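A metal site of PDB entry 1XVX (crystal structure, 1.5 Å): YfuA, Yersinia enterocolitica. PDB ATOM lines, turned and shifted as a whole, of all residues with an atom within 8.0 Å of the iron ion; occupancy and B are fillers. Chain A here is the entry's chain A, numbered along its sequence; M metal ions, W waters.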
ATOM      1  N   ALA A  12      17.411  23.384 -15.361  1.00  0.00           N
ATOM      2  CA  ALA A  12      16.266  23.114 -16.218  1.00  0.00           C
ATOM      3  C   ALA A  12      16.222  24.018 -17.460  1.00  0.00           C
ATOM      4  O   ALA A  12      15.314  23.887 -18.272  1.00  0.00           O
ATOM      5  CB  ALA A  12      14.981  23.225 -15.419  1.00  0.00           C
ATOM      6  N   GLN A  13      17.191  24.923 -17.595  1.00  0.00           N
ATOM      7  CA  GLN A  13      17.305  25.749 -18.804  1.00  0.00           C
ATOM      8  C   GLN A  13      17.973  24.911 -19.915  1.00  0.00           C
ATOM      9  O   GLN A  13      18.621  23.890 -19.619  1.00  0.00           O
ATOM     10  CB  GLN A  13      18.027  27.083 -18.472  1.00  0.00           C
ATOM     11  CG  GLN A  13      18.307  28.099 -19.624  1.00  0.00           C
ATOM     12  CD  GLN A  13      17.087  28.532 -20.449  1.00  0.00           C
ATOM     13  OE1 GLN A  13      16.696  27.844 -21.399  1.00  0.00           O
ATOM     14  NE2 GLN A  13      16.553  29.739 -20.160  1.00  0.00           N
ATOM     15  N   HIS A  14      17.786  25.290 -21.180  1.00  0.00           N
ATOM     16  CA  HIS A  14      18.363  24.536 -22.300  1.00  0.00           C
ATOM     17  C   HIS A  14      19.880  24.390 -22.103  1.00  0.00           C
ATOM     18  O   HIS A  14      20.578  25.367 -21.821  1.00  0.00           O
ATOM     19  CB  HIS A  14      17.998  25.130 -23.668  1.00  0.00           C
ATOM     20  CG  HIS A  14      16.580  24.869 -24.068  1.00  0.00           C
ATOM     21  ND1 HIS A  14      16.172  23.678 -24.654  1.00  0.00           N
ATOM     22  CD2 HIS A  14      15.457  25.628 -23.954  1.00  0.00           C
ATOM     23  CE1 HIS A  14      14.872  23.720 -24.890  1.00  0.00           C
ATOM     24  NE2 HIS A  14      14.410  24.892 -24.463  1.00  0.00           N
ATOM     25  N   ASP A  40      11.869  21.776 -15.751  1.00  0.00           N
ATOM     26  CA  ASP A  40      11.481  22.686 -14.644  1.00  0.00           C
ATOM     27  C   ASP A  40      10.719  21.949 -13.525  1.00  0.00           C
ATOM     28  O   ASP A  40      11.067  22.055 -12.343  1.00  0.00           O
ATOM     29  CB  ASP A  40      10.531  23.803 -15.128  1.00  0.00           C
ATOM     30  CG  ASP A  40      11.227  24.907 -15.939  1.00  0.00           C
ATOM     31  OD1 ASP A  40      12.404  24.764 -16.344  1.00  0.00           O
ATOM     32  OD2 ASP A  40      10.561  25.935 -16.199  1.00  0.00           O
ATOM     33  N   GLU A  62      13.720  27.257 -17.179  1.00  0.00           N
ATOM     34  CA  GLU A  62      13.273  27.891 -18.406  1.00  0.00           C
ATOM     35  C   GLU A  62      12.165  28.908 -18.153  1.00  0.00           C
ATOM     36  O   GLU A  62      12.085  29.917 -18.862  1.00  0.00           O
ATOM     37  CB  GLU A  62      12.736  26.848 -19.369  1.00  0.00           C
ATOM     38  CG  GLU A  62      13.793  26.021 -20.056  1.00  0.00           C
ATOM     39  CD  GLU A  62      13.198  25.268 -21.210  1.00  0.00           C
ATOM     40  OE1 GLU A  62      12.930  25.909 -22.239  1.00  0.00           O
ATOM     41  OE2 GLU A  62      12.979  24.046 -21.062  1.00  0.00           O
ATOM     42  N   ASN A  63      11.305  28.618 -17.167  1.00  0.00           N
ATOM     43  CA  ASN A  63      10.109  29.427 -16.908  1.00  0.00           C
ATOM     44  C   ASN A  63       9.934  29.755 -15.433  1.00  0.00           C
ATOM     45  O   ASN A  63      10.653  29.224 -14.576  1.00  0.00           O
ATOM     46  CB  ASN A  63       8.869  28.687 -17.417  1.00  0.00           C
ATOM     47  CG  ASN A  63       9.028  28.195 -18.843  1.00  0.00           C
ATOM     48  OD1 ASN A  63       8.838  28.949 -19.811  1.00  0.00           O
ATOM     49  ND2 ASN A  63       9.377  26.921 -18.986  1.00  0.00           N
ATOM     50  N   ARG A 104      11.819  34.701 -22.911  1.00  0.00           N
ATOM     51  CA  ARG A 104      11.471  34.123 -24.205  1.00  0.00           C
ATOM     52  C   ARG A 104      10.053  34.572 -24.566  1.00  0.00           C
ATOM     53  O   ARG A 104       9.216  34.762 -23.682  1.00  0.00           O
ATOM     54  CB  ARG A 104      11.597  32.588 -24.156  1.00  0.00           C
ATOM     55  CG  ARG A 104      10.783  31.903 -23.038  1.00  0.00           C
ATOM     56  CD  ARG A 104      11.623  31.654 -21.767  1.00  0.00           C
ATOM     57  NE  ARG A 104      12.726  30.727 -22.017  1.00  0.00           N
ATOM     58  CZ  ARG A 104      12.611  29.402 -22.104  1.00  0.00           C
ATOM     59  NH1 ARG A 104      13.679  28.657 -22.348  1.00  0.00           N
ATOM     60  NH2 ARG A 104      11.411  28.815 -21.957  1.00  0.00           N
ATOM     61  N   ALA A 143       7.205  22.173 -19.482  1.00  0.00           N
ATOM     62  CA  ALA A 143       7.055  23.349 -18.638  1.00  0.00           C
ATOM     63  C   ALA A 143       6.849  24.624 -19.475  1.00  0.00           C
ATOM     64  O   ALA A 143       6.195  25.569 -19.019  1.00  0.00           O
ATOM     65  CB  ALA A 143       8.262  23.511 -17.722  1.00  0.00           C
ATOM     66  N   ASP A 144       7.400  24.633 -20.691  1.00  0.00           N
ATOM     67  CA  ASP A 144       7.258  25.791 -21.581  1.00  0.00           C
ATOM     68  C   ASP A 144       5.789  26.103 -21.866  1.00  0.00           C
ATOM     69  O   ASP A 144       5.296  27.197 -21.563  1.00  0.00           O
ATOM     70  CB  ASP A 144       8.006  25.572 -22.902  1.00  0.00           C
ATOM     71  CG  ASP A 144       9.510  25.784 -22.777  1.00  0.00           C
ATOM     72  OD1 ASP A 144      10.016  26.237 -21.714  1.00  0.00           O
ATOM     73  OD2 ASP A 144      10.189  25.490 -23.787  1.00  0.00           O
ATOM     74  N   PHE A 145       5.089  25.122 -22.445  1.00  0.00           N
ATOM     75  CA  PHE A 145       3.675  25.324 -22.742  1.00  0.00           C
ATOM     76  C   PHE A 145       2.838  25.530 -21.470  1.00  0.00           C
ATOM     77  O   PHE A 145       1.912  26.350 -21.441  1.00  0.00           O
ATOM     78  CB  PHE A 145       3.108  24.158 -23.559  1.00  0.00           C
ATOM     79  CG  PHE A 145       1.694  24.413 -23.999  1.00  0.00           C
ATOM     80  CD1 PHE A 145       1.437  25.230 -25.089  1.00  0.00           C
ATOM     81  CD2 PHE A 145       0.622  23.883 -23.292  1.00  0.00           C
ATOM     82  CE1 PHE A 145       0.127  25.517 -25.484  1.00  0.00           C
ATOM     83  CE2 PHE A 145      -0.677  24.148 -23.670  1.00  0.00           C
ATOM     84  CZ  PHE A 145      -0.937  24.966 -24.773  1.00  0.00           C
ATOM     85  N   GLY A 177       7.913  17.891 -27.130  1.00  0.00           N
ATOM     86  CA  GLY A 177       9.002  18.831 -27.357  1.00  0.00           C
ATOM     87  C   GLY A 177       8.645  19.896 -28.369  1.00  0.00           C
ATOM     88  O   GLY A 177       8.081  19.595 -29.429  1.00  0.00           O
ATOM     89  N   ASN A 178       8.975  21.141 -28.036  1.00  0.00           N
ATOM     90  CA  ASN A 178       8.747  22.255 -28.964  1.00  0.00           C
ATOM     91  C   ASN A 178       9.557  22.181 -30.252  1.00  0.00           C
ATOM     92  O   ASN A 178       9.099  22.629 -31.294  1.00  0.00           O
ATOM     93  CB  ASN A 178       8.974  23.603 -28.271  1.00  0.00           C
ATOM     94  CG  ASN A 178       7.934  23.873 -27.205  1.00  0.00           C
ATOM     95  OD1 ASN A 178       6.754  23.545 -27.381  1.00  0.00           O
ATOM     96  ND2 ASN A 178       8.367  24.465 -26.092  1.00  0.00           N
ATOM     97  N   SER A 179      10.749  21.596 -30.192  1.00  0.00           N
ATOM     98  CA  SER A 179      11.516  21.358 -31.424  1.00  0.00           C
ATOM     99  C   SER A 179      10.753  20.420 -32.351  1.00  0.00           C
ATOM    100  O   SER A 179      10.765  20.597 -33.570  1.00  0.00           O
ATOM    101  CB  SER A 179      12.909  20.805 -31.117  1.00  0.00           C
ATOM    102  OG  SER A 179      12.813  19.548 -30.497  1.00  0.00           O
ATOM    103  N   ILE A 195       4.709  27.745 -29.627  1.00  0.00           N
ATOM    104  CA  ILE A 195       6.024  27.451 -29.048  1.00  0.00           C
ATOM    105  C   ILE A 195       6.643  28.751 -28.524  1.00  0.00           C
ATOM    106  O   ILE A 195       5.941  29.760 -28.441  1.00  0.00           O
ATOM    107  CB  ILE A 195       6.979  26.695 -30.046  1.00  0.00           C
ATOM    108  CG1 ILE A 195       7.327  27.554 -31.265  1.00  0.00           C
ATOM    109  CG2 ILE A 195       6.361  25.336 -30.472  1.00  0.00           C
ATOM    110  CD1 ILE A 195       8.461  27.005 -32.164  1.00  0.00           C
ATOM    111  N   TYR A 196       7.923  28.719 -28.162  1.00  0.00           N
ATOM    112  CA  TYR A 196       8.665  29.956 -27.882  1.00  0.00           C
ATOM    113  C   TYR A 196       9.542  30.343 -29.057  1.00  0.00           C
ATOM    114  O   TYR A 196       9.904  29.500 -29.889  1.00  0.00           O
ATOM    115  CB  TYR A 196       9.514  29.837 -26.609  1.00  0.00           C
ATOM    116  CG  TYR A 196       8.702  29.850 -25.326  1.00  0.00           C
ATOM    117  CD1 TYR A 196       7.705  30.826 -25.096  1.00  0.00           C
ATOM    118  CD2 TYR A 196       8.939  28.911 -24.325  1.00  0.00           C
ATOM    119  CE1 TYR A 196       6.963  30.845 -23.901  1.00  0.00           C
ATOM    120  CE2 TYR A 196       8.200  28.929 -23.116  1.00  0.00           C
ATOM    121  CZ  TYR A 196       7.221  29.887 -22.923  1.00  0.00           C
ATOM    122  OH  TYR A 196       6.497  29.897 -21.742  1.00  0.00           O
ATOM    123  N   TYR A 198      12.695  31.131 -29.567  1.00  0.00           N
ATOM    124  CA  TYR A 198      14.126  30.812 -29.769  1.00  0.00           C
ATOM    125  C   TYR A 198      14.375  29.551 -30.600  1.00  0.00           C
ATOM    126  O   TYR A 198      15.412  29.455 -31.247  1.00  0.00           O
ATOM    127  CB  TYR A 198      14.885  30.730 -28.428  1.00  0.00           C
ATOM    128  CG  TYR A 198      14.236  29.790 -27.444  1.00  0.00           C
ATOM    129  CD1 TYR A 198      14.512  28.427 -27.462  1.00  0.00           C
ATOM    130  CD2 TYR A 198      13.335  30.269 -26.505  1.00  0.00           C
ATOM    131  CE1 TYR A 198      13.898  27.554 -26.557  1.00  0.00           C
ATOM    132  CE2 TYR A 198      12.718  29.416 -25.612  1.00  0.00           C
ATOM    133  CZ  TYR A 198      13.000  28.074 -25.636  1.00  0.00           C
ATOM    134  OH  TYR A 198      12.361  27.262 -24.740  1.00  0.00           O
ATOM    135  N   TYR A 199      13.431  28.617 -30.603  1.00  0.00           N
ATOM    136  CA  TYR A 199      13.650  27.367 -31.312  1.00  0.00           C
ATOM    137  C   TYR A 199      14.044  27.574 -32.779  1.00  0.00           C
ATOM    138  O   TYR A 199      15.005  26.952 -33.254  1.00  0.00           O
ATOM    139  CB  TYR A 199      12.422  26.453 -31.203  1.00  0.00           C
ATOM    140  CG  TYR A 199      12.216  25.915 -29.818  1.00  0.00           C
ATOM    141  CD1 TYR A 199      12.879  24.753 -29.400  1.00  0.00           C
ATOM    142  CD2 TYR A 199      11.362  26.557 -28.922  1.00  0.00           C
ATOM    143  CE1 TYR A 199      12.684  24.235 -28.121  1.00  0.00           C
ATOM    144  CE2 TYR A 199      11.173  26.057 -27.628  1.00  0.00           C
ATOM    145  CZ  TYR A 199      11.827  24.897 -27.236  1.00  0.00           C
ATOM    146  OH  TYR A 199      11.621  24.401 -25.974  1.00  0.00           O
ATOM    147  N   GLU A 268      17.984  33.558 -26.643  1.00  0.00           N
ATOM    148  CA  GLU A 268      17.001  34.015 -25.658  1.00  0.00           C
ATOM    149  C   GLU A 268      17.279  35.467 -25.259  1.00  0.00           C
ATOM    150  O   GLU A 268      18.387  35.960 -25.440  1.00  0.00           O
ATOM    151  CB  GLU A 268      16.919  33.048 -24.465  1.00  0.00           C
ATOM    152  CG  GLU A 268      16.546  31.625 -24.935  1.00  0.00           C
ATOM    153  CD  GLU A 268      16.219  30.643 -23.816  1.00  0.00           C
ATOM    154  OE1 GLU A 268      15.695  31.061 -22.783  1.00  0.00           O
ATOM    155  OE2 GLU A 268      16.482  29.426 -24.001  1.00  0.00           O
HETATM  156 FE    FE M   1      12.260  25.299 -24.195  1.00  0.00          FE
HETATM  157  O   HOH W   1      12.061  23.338 -23.293  1.00  0.00           O
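The side-chain hydroxyl (OH) of Tyr 198 lies close to the guanidinium group (NH1) of Arg 104 (3.1 Å). OH of Tyr 199 sits close to ND2 of Asn 178 (3.3 Å). The side-chain carboxylate (OD1) of Asp 144 is in salt-bridge range of the guanidinium group (NH2) of Arg 104. OD2 of Asp 144 sits close to ND2 of Asn 178, at 3.1 Å. The backbone carbonyl oxygen of Asp 144 lies within hydrogen-bond range of the side-chain hydroxyl of Tyr 196 (3.0 Å). The side-chain carboxylate (OD1) of Asp 144 lies within hydrogen-bond range of the side-chain amide nitrogen (ND2) of Asn 63 (2.9 Å). NE of Arg 104 is in hydrogen-bond range of O of Glu 62, 3.3 Å away. The backbone NH (N) of Glu 62 sits at hydrogen-bond distance from the side-chain carboxylate (OD1) of Asp 40 (2.9 Å).
Within 4 Å of the iron ion: His 14, Glu 62, Asp 144, Tyr 198 and Tyr 199. Along chain A the residues within 4 Å of the iron ion span positions 14 to 199. The nearest printed residue that does not touch the iron ion is Arg 104 (4.1 Å).
The iron ion is bound by OH of Tyr 198, at 2.0 Å. The side-chain hydroxyl (OH) of Tyr 199 binds the iron ion (2.1 Å). The iron ion is bound by OD2 of Asp 144. OE1 of Glu 62 is bound to the iron ion (2.2 Å). Water W1 is bound to the iron ion. NE2 of His 14 is bound to the iron ion, 2.2 Å away.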
